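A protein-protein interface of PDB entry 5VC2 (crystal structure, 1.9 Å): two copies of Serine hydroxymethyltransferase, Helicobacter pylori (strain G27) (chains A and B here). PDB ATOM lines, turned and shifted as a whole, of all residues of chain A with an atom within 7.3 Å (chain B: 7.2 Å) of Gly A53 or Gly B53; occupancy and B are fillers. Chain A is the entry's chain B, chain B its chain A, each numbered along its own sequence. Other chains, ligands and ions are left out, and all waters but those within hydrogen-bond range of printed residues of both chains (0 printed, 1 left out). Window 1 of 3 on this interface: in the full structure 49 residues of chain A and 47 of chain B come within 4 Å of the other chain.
O of Gly B53 sits at hydrogen-bond distance from N of Phe A424 (3.0 Å). O of Pro A422 is in hydrogen-bond range of N of Ile B55 (3.0 Å). The backbone NH (N) of Ile A55 lies within hydrogen-bond range of the backbone carbonyl oxygen (O) of Pro B422 (3.0 Å). N of Phe B424 lies within hydrogen-bond range of O of Gly A53 (3.0 Å). O of Phe B424 sits close to O of Phe A424 (2.7 Å). The backbone carbonyl oxygen of Ser B54 lies close to the side-chain sulfur of Met A49 (3.6 Å). The side-chain sulfur of Met B49 sits close to the backbone carbonyl oxygen of Ser A54, at 3.5 Å.
The backbone carbonyl oxygen (O) of Ala B51 sits at hydrogen-bond distance from the side-chain hydroxyl (OG) of Ser B54, 2.8 Å away. N of Leu B56 lies close to OG of Ser B54 (3.3 Å). The side-chain hydroxyl (OG) of Ser A54 is in hydrogen-bond range of the backbone carbonyl oxygen (O) of Ala A51. OG of Ser A54 lies close to N of Leu A56 (3.2 Å).
Gly B53 touches Met A49. Ile B55 touches Met A49 (CA to SD, 3.8 Å). Met A49 touches Thr B57 (SD to CG2, 3.8 Å). Met B49 touches Gly A53 (O to CA, 3.4 Å). Gly A53 touches Ile B423 (O to C, 3.96 Å). Pro B422 touches Ser A54 (O to CA, 3.3 Å). CE1 of Phe B424 touches CG2 of Ile A55 (3.98 Å). Gly B53 touches Ile A423. Ser B54 touches Ile A423 (CB to CG1, 3.9 Å). Phe A424 touches Ile B55 (CE1 to CG2, 3.97 Å).
Of the printed residues of chain B, Met A52 touches Met B52. Printed residues of chain B within 4 Å of Gly A53: Met B49, Gly B53, Ile B423 and Phe B424. Printed residues of chain A within 4 Å of Glu B50: Ile A423 (3.4 Å). Of the printed residues of chain A, Met B52 touches Met A52 (3.6 Å). Printed residues of chain A within 4 Å of Gly B53: Met A49 (3.5 Å), Gly A53 (3.8 Å), Ile A423 (3.99 Å) and Phe A424 (3.0 Å). Printed residues of chain A within 4 Å of Ser B54: Met A49 (3.6 Å), Pro A422 (3.5 Å) and Ile A423 (3.9 Å). His B270 touches none of the printed residues of chain A. Printed residues of chain A within 4 Å of Ile B423: Glu A50, Gly A53 and Phe A424. The nearest residue of chain B that does not touch Gly A53 is Met B52 (4.4 Å).
Printed residues of chain A that touch a printed residue of chain B: Met A49, Glu A50, Met A52, Gly A53, Ser A54, Ile A55, Thr A57, Pro A422, Ile A423 and Phe A424. Hydrophobic or aromatic side chains of chain A that line the printed part of chain B: Met A49, Met A52, Ile A55, Ile A423 and Phe A424. Among the printed residues, 26 pairs touch across the chains.
Met A49 touches Thr B57, and with the chains exchanged Thr A57 touches Met B49. Gly B53 touches its own counterpart, Gly A53. Gly A53 touches Phe B424, and with the chains exchanged Phe A424 touches Gly B53. Ile A423 touches Ser B54, but with the chains exchanged Ser A54 does not touch Ile B423 (4.1 Å). Positions printed for both chains: 46, 47, 48, 49, 50, 51, 52, 53, 54, 55, 56, 57, 270, 274, 422, 423 and 424. Of the 26 pairs that touch across the chains among the printed residues, 25 have their exchanged pair printed and touching as well.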
ATOM      1  N   PRO A  46      10.067 -19.129 -21.642  1.00  0.00           N
ATOM      2  CA  PRO A  46      11.403 -18.814 -22.184  1.00  0.00           C
ATOM      3  C   PRO A  46      12.358 -18.221 -21.162  1.00  0.00           C
ATOM      4  O   PRO A  46      13.539 -18.591 -21.140  1.00  0.00           O
ATOM      5  CB  PRO A  46      11.095 -17.808 -23.310  1.00  0.00           C
ATOM      6  CG  PRO A  46       9.676 -18.088 -23.706  1.00  0.00           C
ATOM      7  CD  PRO A  46       8.978 -18.532 -22.445  1.00  0.00           C
ATOM      8  N   SER A  47      11.883 -17.304 -20.308  1.00  0.00           N
ATOM      9  CA  SER A  47      12.774 -16.701 -19.319  1.00  0.00           C
ATOM     10  C   SER A  47      13.322 -17.732 -18.336  1.00  0.00           C
ATOM     11  O   SER A  47      14.433 -17.563 -17.814  1.00  0.00           O
ATOM     12  CB  SER A  47      12.042 -15.578 -18.581  1.00  0.00           C
ATOM     13  OG  SER A  47      10.916 -16.106 -17.896  1.00  0.00           O
ATOM     14  N   VAL A  48      12.566 -18.801 -18.063  1.00  0.00           N
ATOM     15  CA  VAL A  48      13.054 -19.850 -17.176  1.00  0.00           C
ATOM     16  C   VAL A  48      14.224 -20.590 -17.814  1.00  0.00           C
ATOM     17  O   VAL A  48      15.232 -20.878 -17.152  1.00  0.00           O
ATOM     18  CB  VAL A  48      11.910 -20.820 -16.806  1.00  0.00           C
ATOM     19  CG1 VAL A  48      12.477 -22.085 -16.188  1.00  0.00           C
ATOM     20  CG2 VAL A  48      10.936 -20.174 -15.847  1.00  0.00           C
ATOM     21  N   MET A  49      14.118 -20.904 -19.111  1.00  0.00           N
ATOM     22  CA  MET A  49      15.248 -21.534 -19.791  1.00  0.00           C
ATOM     23  C   MET A  49      16.457 -20.607 -19.842  1.00  0.00           C
ATOM     24  O   MET A  49      17.599 -21.076 -19.777  1.00  0.00           O
ATOM     25  CB  MET A  49      14.826 -21.979 -21.197  1.00  0.00           C
ATOM     26  CG  MET A  49      13.877 -23.184 -21.147  1.00  0.00           C
ATOM     27  SD  MET A  49      13.256 -23.749 -22.744  1.00  0.00           S
ATOM     28  CE  MET A  49      12.079 -22.433 -23.065  1.00  0.00           C
ATOM     29  N   GLU A  50      16.244 -19.293 -19.937  1.00  0.00           N
ATOM     30  CA  GLU A  50      17.388 -18.381 -19.893  1.00  0.00           C
ATOM     31  C   GLU A  50      18.139 -18.522 -18.581  1.00  0.00           C
ATOM     32  O   GLU A  50      19.371 -18.621 -18.569  1.00  0.00           O
ATOM     33  CB  GLU A  50      16.951 -16.927 -20.096  1.00  0.00           C
ATOM     34  CG  GLU A  50      16.522 -16.627 -21.497  1.00  0.00           C
ATOM     35  CD  GLU A  50      16.044 -15.196 -21.688  1.00  0.00           C
ATOM     36  OE1 GLU A  50      16.233 -14.354 -20.776  1.00  0.00           O
ATOM     37  OE2 GLU A  50      15.479 -14.926 -22.767  1.00  0.00           O
ATOM     38  N   ALA A  51      17.411 -18.559 -17.455  1.00  0.00           N
ATOM     39  CA  ALA A  51      18.071 -18.801 -16.173  1.00  0.00           C
ATOM     40  C   ALA A  51      18.799 -20.141 -16.166  1.00  0.00           C
ATOM     41  O   ALA A  51      19.897 -20.262 -15.603  1.00  0.00           O
ATOM     42  CB  ALA A  51      17.045 -18.749 -15.032  1.00  0.00           C
ATOM     43  N   MET A  52      18.182 -21.171 -16.750  1.00  0.00           N
ATOM     44  CA  MET A  52      18.800 -22.499 -16.776  1.00  0.00           C
ATOM     45  C   MET A  52      20.116 -22.507 -17.543  1.00  0.00           C
ATOM     46  O   MET A  52      21.031 -23.285 -17.209  1.00  0.00           O
ATOM     47  CB  MET A  52      17.841 -23.502 -17.409  1.00  0.00           C
ATOM     48  CG  MET A  52      16.644 -23.809 -16.545  1.00  0.00           C
ATOM     49  SD  MET A  52      17.082 -24.828 -15.115  1.00  0.00           S
ATOM     50  CE  MET A  52      18.382 -25.844 -15.742  1.00  0.00           C
ATOM     51  N   GLY A  53      20.220 -21.683 -18.581  1.00  0.00           N
ATOM     52  CA  GLY A  53      21.426 -21.606 -19.398  1.00  0.00           C
ATOM     53  C   GLY A  53      22.378 -20.481 -19.014  1.00  0.00           C
ATOM     54  O   GLY A  53      23.221 -20.076 -19.824  1.00  0.00           O
ATOM     55  N   SER A  54      22.270 -19.978 -17.785  1.00  0.00           N
ATOM     56  CA  SER A  54      23.080 -18.851 -17.331  1.00  0.00           C
ATOM     57  C   SER A  54      24.374 -19.306 -16.647  1.00  0.00           C
ATOM     58  O   SER A  54      24.576 -20.487 -16.344  1.00  0.00           O
ATOM     59  CB  SER A  54      22.280 -17.975 -16.369  1.00  0.00           C
ATOM     60  OG  SER A  54      22.204 -18.586 -15.082  1.00  0.00           O
ATOM     61  N   ILE A  55      25.244 -18.332 -16.358  1.00  0.00           N
ATOM     62  CA  ILE A  55      26.536 -18.613 -15.735  1.00  0.00           C
ATOM     63  C   ILE A  55      26.357 -19.011 -14.276  1.00  0.00           C
ATOM     64  O   ILE A  55      27.337 -19.303 -13.583  1.00  0.00           O
ATOM     65  CB  ILE A  55      27.519 -17.425 -15.886  1.00  0.00           C
ATOM     66  CG1 ILE A  55      26.903 -16.062 -15.489  1.00  0.00           C
ATOM     67  CG2 ILE A  55      27.978 -17.341 -17.325  1.00  0.00           C
ATOM     68  CD1 ILE A  55      26.672 -15.857 -14.010  1.00  0.00           C
ATOM     69  N   LEU A  56      25.116 -19.017 -13.783  1.00  0.00           N
ATOM     70  CA  LEU A  56      24.901 -19.465 -12.407  1.00  0.00           C
ATOM     71  C   LEU A  56      25.294 -20.920 -12.212  1.00  0.00           C
ATOM     72  O   LEU A  56      25.505 -21.348 -11.071  1.00  0.00           O
ATOM     73  CB  LEU A  56      23.443 -19.271 -11.994  1.00  0.00           C
ATOM     74  CG  LEU A  56      22.966 -17.822 -11.934  1.00  0.00           C
ATOM     75  CD1 LEU A  56      21.464 -17.805 -11.584  1.00  0.00           C
ATOM     76  CD2 LEU A  56      23.768 -17.035 -10.900  1.00  0.00           C
ATOM     77  N   THR A  57      25.400 -21.688 -13.294  1.00  0.00           N
ATOM     78  CA  THR A  57      25.876 -23.060 -13.165  1.00  0.00           C
ATOM     79  C   THR A  57      27.280 -23.136 -12.564  1.00  0.00           C
ATOM     80  O   THR A  57      27.617 -24.156 -11.956  1.00  0.00           O
ATOM     81  CB  THR A  57      25.834 -23.762 -14.524  1.00  0.00           C
ATOM     82  OG1 THR A  57      26.230 -25.125 -14.368  1.00  0.00           O
ATOM     83  CG2 THR A  57      26.770 -23.099 -15.484  1.00  0.00           C
ATOM     84  N   HIS A 270      21.545 -22.195 -10.845  1.00  0.00           N
ATOM     85  CA  HIS A 270      20.783 -21.923 -12.059  1.00  0.00           C
ATOM     86  C   HIS A 270      19.374 -22.506 -11.971  1.00  0.00           C
ATOM     87  O   HIS A 270      18.412 -21.882 -12.436  1.00  0.00           O
ATOM     88  CB  HIS A 270      21.528 -22.452 -13.281  1.00  0.00           C
ATOM     89  CG  HIS A 270      21.905 -23.900 -13.181  1.00  0.00           C
ATOM     90  ND1 HIS A 270      22.779 -24.377 -12.230  1.00  0.00           N
ATOM     91  CD2 HIS A 270      21.547 -24.968 -13.933  1.00  0.00           C
ATOM     92  CE1 HIS A 270      22.936 -25.679 -12.391  1.00  0.00           C
ATOM     93  NE2 HIS A 270      22.200 -26.062 -13.417  1.00  0.00           N
ATOM     94  N   ALA A 274      15.937 -20.429 -11.794  1.00  0.00           N
ATOM     95  CA  ALA A 274      14.874 -20.747 -12.742  1.00  0.00           C
ATOM     96  C   ALA A 274      13.528 -20.917 -12.039  1.00  0.00           C
ATOM     97  O   ALA A 274      12.496 -20.466 -12.552  1.00  0.00           O
ATOM     98  CB  ALA A 274      15.242 -22.016 -13.523  1.00  0.00           C
ATOM     99  N   PRO A 422      15.172 -22.414 -30.425  1.00  0.00           N
ATOM    100  CA  PRO A 422      15.314 -23.676 -29.681  1.00  0.00           C
ATOM    101  C   PRO A 422      16.229 -23.581 -28.462  1.00  0.00           C
ATOM    102  O   PRO A 422      16.233 -24.473 -27.604  1.00  0.00           O
ATOM    103  CB  PRO A 422      15.900 -24.617 -30.735  1.00  0.00           C
ATOM    104  CG  PRO A 422      16.807 -23.697 -31.549  1.00  0.00           C
ATOM    105  CD  PRO A 422      16.154 -22.318 -31.526  1.00  0.00           C
ATOM    106  N   ILE A 423      17.029 -22.523 -28.374  1.00  0.00           N
ATOM    107  CA  ILE A 423      17.979 -22.356 -27.280  1.00  0.00           C
ATOM    108  C   ILE A 423      17.841 -20.945 -26.731  1.00  0.00           C
ATOM    109  O   ILE A 423      17.864 -19.971 -27.493  1.00  0.00           O
ATOM    110  CB  ILE A 423      19.430 -22.625 -27.729  1.00  0.00           C
ATOM    111  CG1 ILE A 423      19.626 -24.109 -28.077  1.00  0.00           C
ATOM    112  CG2 ILE A 423      20.402 -22.164 -26.662  1.00  0.00           C
ATOM    113  CD1 ILE A 423      20.920 -24.402 -28.828  1.00  0.00           C
ATOM    114  N   PHE A 424      17.703 -20.837 -25.414  1.00  0.00           N
ATOM    115  CA  PHE A 424      17.589 -19.544 -24.754  1.00  0.00           C
ATOM    116  C   PHE A 424      18.812 -19.251 -23.891  1.00  0.00           C
ATOM    117  O   PHE A 424      19.470 -18.226 -24.059  1.00  0.00           O
ATOM    118  CB  PHE A 424      16.310 -19.497 -23.920  1.00  0.00           C
ATOM    119  CG  PHE A 424      15.061 -19.623 -24.741  1.00  0.00           C
ATOM    120  CD1 PHE A 424      14.571 -20.872 -25.100  1.00  0.00           C
ATOM    121  CD2 PHE A 424      14.390 -18.490 -25.185  1.00  0.00           C
ATOM    122  CE1 PHE A 424      13.412 -20.987 -25.876  1.00  0.00           C
ATOM    123  CE2 PHE A 424      13.237 -18.601 -25.961  1.00  0.00           C
ATOM    124  CZ  PHE A 424      12.749 -19.850 -26.304  1.00  0.00           C
ATOM    125  OXT PHE A 424      19.181 -20.031 -23.015  1.00  0.00           O
ATOM    126  N   PRO B  46      30.701 -22.530 -22.845  1.00  0.00           N
ATOM    127  CA  PRO B  46      29.484 -21.861 -23.332  1.00  0.00           C
ATOM    128  C   PRO B  46      28.496 -22.788 -24.038  1.00  0.00           C
ATOM    129  O   PRO B  46      27.285 -22.660 -23.827  1.00  0.00           O
ATOM    130  CB  PRO B  46      30.051 -20.792 -24.284  1.00  0.00           C
ATOM    131  CG  PRO B  46      31.382 -20.442 -23.675  1.00  0.00           C
ATOM    132  CD  PRO B  46      31.922 -21.767 -23.170  1.00  0.00           C
ATOM    133  N   SER B  47      28.967 -23.730 -24.862  1.00  0.00           N
ATOM    134  CA  SER B  47      28.026 -24.603 -25.564  1.00  0.00           C
ATOM    135  C   SER B  47      27.289 -25.532 -24.608  1.00  0.00           C
ATOM    136  O   SER B  47      26.164 -25.959 -24.905  1.00  0.00           O
ATOM    137  CB  SER B  47      28.757 -25.425 -26.625  1.00  0.00           C
ATOM    138  OG  SER B  47      29.799 -26.142 -26.009  1.00  0.00           O
ATOM    139  N   VAL B  48      27.906 -25.873 -23.473  1.00  0.00           N
ATOM    140  CA  VAL B  48      27.206 -26.663 -22.461  1.00  0.00           C
ATOM    141  C   VAL B  48      26.043 -25.877 -21.886  1.00  0.00           C
ATOM    142  O   VAL B  48      24.949 -26.422 -21.662  1.00  0.00           O
ATOM    143  CB  VAL B  48      28.179 -27.115 -21.356  1.00  0.00           C
ATOM    144  CG1 VAL B  48      27.408 -27.652 -20.159  1.00  0.00           C
ATOM    145  CG2 VAL B  48      29.134 -28.172 -21.887  1.00  0.00           C
ATOM    146  N   MET B  49      26.259 -24.584 -21.618  1.00  0.00           N
ATOM    147  CA  MET B  49      25.174 -23.767 -21.094  1.00  0.00           C
ATOM    148  C   MET B  49      24.062 -23.584 -22.119  1.00  0.00           C
ATOM    149  O   MET B  49      22.888 -23.546 -21.741  1.00  0.00           O
ATOM    150  CB  MET B  49      25.736 -22.412 -20.610  1.00  0.00           C
ATOM    151  CG  MET B  49      26.533 -22.571 -19.294  1.00  0.00           C
ATOM    152  SD  MET B  49      27.215 -21.000 -18.662  1.00  0.00           S
ATOM    153  CE  MET B  49      28.520 -20.737 -19.846  1.00  0.00           C
ATOM    154  N   GLU B  50      24.393 -23.514 -23.418  1.00  0.00           N
ATOM    155  CA  GLU B  50      23.337 -23.464 -24.429  1.00  0.00           C
ATOM    156  C   GLU B  50      22.451 -24.704 -24.355  1.00  0.00           C
ATOM    157  O   GLU B  50      21.221 -24.599 -24.391  1.00  0.00           O
ATOM    158  CB  GLU B  50      23.918 -23.334 -25.841  1.00  0.00           C
ATOM    159  CG  GLU B  50      24.640 -22.056 -26.132  1.00  0.00           C
ATOM    160  CD  GLU B  50      25.037 -21.946 -27.595  1.00  0.00           C
ATOM    161  OE1 GLU B  50      24.904 -22.944 -28.336  1.00  0.00           O
ATOM    162  OE2 GLU B  50      25.470 -20.851 -27.999  1.00  0.00           O
ATOM    163  N   ALA B  51      23.062 -25.889 -24.253  1.00  0.00           N
ATOM    164  CA  ALA B  51      22.277 -27.115 -24.100  1.00  0.00           C
ATOM    165  C   ALA B  51      21.435 -27.075 -22.827  1.00  0.00           C
ATOM    166  O   ALA B  51      20.269 -27.488 -22.834  1.00  0.00           O
ATOM    167  CB  ALA B  51      23.203 -28.331 -24.077  1.00  0.00           C
ATOM    168  N   MET B  52      22.020 -26.590 -21.722  1.00  0.00           N
ATOM    169  CA  MET B  52      21.277 -26.476 -20.460  1.00  0.00           C
ATOM    170  C   MET B  52      20.063 -25.567 -20.599  1.00  0.00           C
ATOM    171  O   MET B  52      19.041 -25.792 -19.932  1.00  0.00           O
ATOM    172  CB  MET B  52      22.172 -25.920 -19.342  1.00  0.00           C
ATOM    173  CG  MET B  52      23.287 -26.840 -18.830  1.00  0.00           C
ATOM    174  SD  MET B  52      22.707 -28.340 -17.984  1.00  0.00           S
ATOM    175  CE  MET B  52      21.239 -27.785 -17.157  1.00  0.00           C
ATOM    176  N   GLY B  53      20.164 -24.531 -21.432  1.00  0.00           N
ATOM    177  CA  GLY B  53      19.063 -23.600 -21.623  1.00  0.00           C
ATOM    178  C   GLY B  53      18.201 -23.904 -22.837  1.00  0.00           C
ATOM    179  O   GLY B  53      17.502 -23.019 -23.338  1.00  0.00           O
ATOM    180  N   SER B  54      18.217 -25.150 -23.309  1.00  0.00           N
ATOM    181  CA  SER B  54      17.499 -25.497 -24.526  1.00  0.00           C
ATOM    182  C   SER B  54      16.098 -26.016 -24.215  1.00  0.00           C
ATOM    183  O   SER B  54      15.745 -26.303 -23.069  1.00  0.00           O
ATOM    184  CB  SER B  54      18.269 -26.546 -25.327  1.00  0.00           C
ATOM    185  OG  SER B  54      18.211 -27.810 -24.674  1.00  0.00           O
ATOM    186  N   ILE B  55      15.296 -26.152 -25.274  1.00  0.00           N
ATOM    187  CA  ILE B  55      13.920 -26.631 -25.177  1.00  0.00           C
ATOM    188  C   ILE B  55      13.879 -28.117 -24.824  1.00  0.00           C
ATOM    189  O   ILE B  55      12.800 -28.678 -24.611  1.00  0.00           O
ATOM    190  CB  ILE B  55      13.146 -26.353 -26.484  1.00  0.00           C
ATOM    191  CG1 ILE B  55      13.916 -26.862 -27.706  1.00  0.00           C
ATOM    192  CG2 ILE B  55      12.891 -24.849 -26.639  1.00  0.00           C
ATOM    193  CD1 ILE B  55      13.745 -28.342 -28.019  1.00  0.00           C
ATOM    194  N   LEU B  56      15.042 -28.769 -24.734  1.00  0.00           N
ATOM    195  CA  LEU B  56      15.039 -30.163 -24.288  1.00  0.00           C
ATOM    196  C   LEU B  56      14.473 -30.311 -22.878  1.00  0.00           C
ATOM    197  O   LEU B  56      14.114 -31.423 -22.476  1.00  0.00           O
ATOM    198  CB  LEU B  56      16.440 -30.760 -24.337  1.00  0.00           C
ATOM    199  CG  LEU B  56      17.061 -30.952 -25.723  1.00  0.00           C
ATOM    200  CD1 LEU B  56      18.471 -31.495 -25.573  1.00  0.00           C
ATOM    201  CD2 LEU B  56      16.235 -31.898 -26.579  1.00  0.00           C
ATOM    202  N   THR B  57      14.365 -29.216 -22.129  1.00  0.00           N
ATOM    203  CA  THR B  57      13.790 -29.310 -20.793  1.00  0.00           C
ATOM    204  C   THR B  57      12.324 -29.728 -20.813  1.00  0.00           C
ATOM    205  O   THR B  57      11.833 -30.261 -19.809  1.00  0.00           O
ATOM    206  CB  THR B  57      13.942 -27.984 -20.051  1.00  0.00           C
ATOM    207  OG1 THR B  57      13.621 -28.184 -18.672  1.00  0.00           O
ATOM    208  CG2 THR B  57      13.011 -26.945 -20.637  1.00  0.00           C
ATOM    209  N   HIS B 270      17.894 -32.064 -21.237  1.00  0.00           N
ATOM    210  CA  HIS B 270      18.814 -30.942 -21.433  1.00  0.00           C
ATOM    211  C   HIS B 270      20.132 -31.157 -20.689  1.00  0.00           C
ATOM    212  O   HIS B 270      21.185 -30.724 -21.169  1.00  0.00           O
ATOM    213  CB  HIS B 270      18.162 -29.622 -20.993  1.00  0.00           C
ATOM    214  CG  HIS B 270      17.615 -29.645 -19.600  1.00  0.00           C
ATOM    215  ND1 HIS B 270      16.579 -30.470 -19.220  1.00  0.00           N
ATOM    216  CD2 HIS B 270      17.972 -28.955 -18.490  1.00  0.00           C
ATOM    217  CE1 HIS B 270      16.303 -30.269 -17.942  1.00  0.00           C
ATOM    218  NE2 HIS B 270      17.141 -29.365 -17.473  1.00  0.00           N
ATOM    219  N   ALA B 274      23.738 -31.758 -22.362  1.00  0.00           N
ATOM    220  CA  ALA B 274      24.847 -30.926 -21.906  1.00  0.00           C
ATOM    221  C   ALA B 274      26.078 -31.761 -21.574  1.00  0.00           C
ATOM    222  O   ALA B 274      27.218 -31.340 -21.838  1.00  0.00           O
ATOM    223  CB  ALA B 274      24.413 -30.110 -20.689  1.00  0.00           C
ATOM    224  N   PRO B 422      26.183 -13.253 -19.898  1.00  0.00           N
ATOM    225  CA  PRO B 422      25.839 -14.048 -18.709  1.00  0.00           C
ATOM    226  C   PRO B 422      24.812 -15.155 -18.961  1.00  0.00           C
ATOM    227  O   PRO B 422      24.611 -16.028 -18.107  1.00  0.00           O
ATOM    228  CB  PRO B 422      25.267 -12.988 -17.757  1.00  0.00           C
ATOM    229  CG  PRO B 422      24.582 -12.012 -18.689  1.00  0.00           C
ATOM    230  CD  PRO B 422      25.422 -11.987 -19.958  1.00  0.00           C
ATOM    231  N   ILE B 423      24.137 -15.119 -20.108  1.00  0.00           N
ATOM    232  CA  ILE B 423      23.092 -16.082 -20.439  1.00  0.00           C
ATOM    233  C   ILE B 423      23.381 -16.657 -21.819  1.00  0.00           C
ATOM    234  O   ILE B 423      23.611 -15.904 -22.773  1.00  0.00           O
ATOM    235  CB  ILE B 423      21.688 -15.443 -20.404  1.00  0.00           C
ATOM    236  CG1 ILE B 423      21.357 -14.933 -18.995  1.00  0.00           C
ATOM    237  CG2 ILE B 423      20.626 -16.429 -20.904  1.00  0.00           C
ATOM    238  CD1 ILE B 423      20.112 -14.038 -18.957  1.00  0.00           C
ATOM    239  N   PHE B 424      23.363 -17.985 -21.921  1.00  0.00           N
ATOM    240  CA  PHE B 424      23.638 -18.679 -23.174  1.00  0.00           C
ATOM    241  C   PHE B 424      22.423 -19.488 -23.620  1.00  0.00           C
ATOM    242  O   PHE B 424      21.894 -19.299 -24.716  1.00  0.00           O
ATOM    243  CB  PHE B 424      24.865 -19.588 -23.021  1.00  0.00           C
ATOM    244  CG  PHE B 424      26.149 -18.842 -22.781  1.00  0.00           C
ATOM    245  CD1 PHE B 424      26.524 -18.462 -21.498  1.00  0.00           C
ATOM    246  CD2 PHE B 424      26.983 -18.508 -23.840  1.00  0.00           C
ATOM    247  CE1 PHE B 424      27.713 -17.761 -21.275  1.00  0.00           C
ATOM    248  CE2 PHE B 424      28.175 -17.813 -23.620  1.00  0.00           C
ATOM    249  CZ  PHE B 424      28.540 -17.445 -22.338  1.00  0.00           C
ATOM    250  OXT PHE B 424      21.927 -20.347 -22.894  1.00  0.00           O
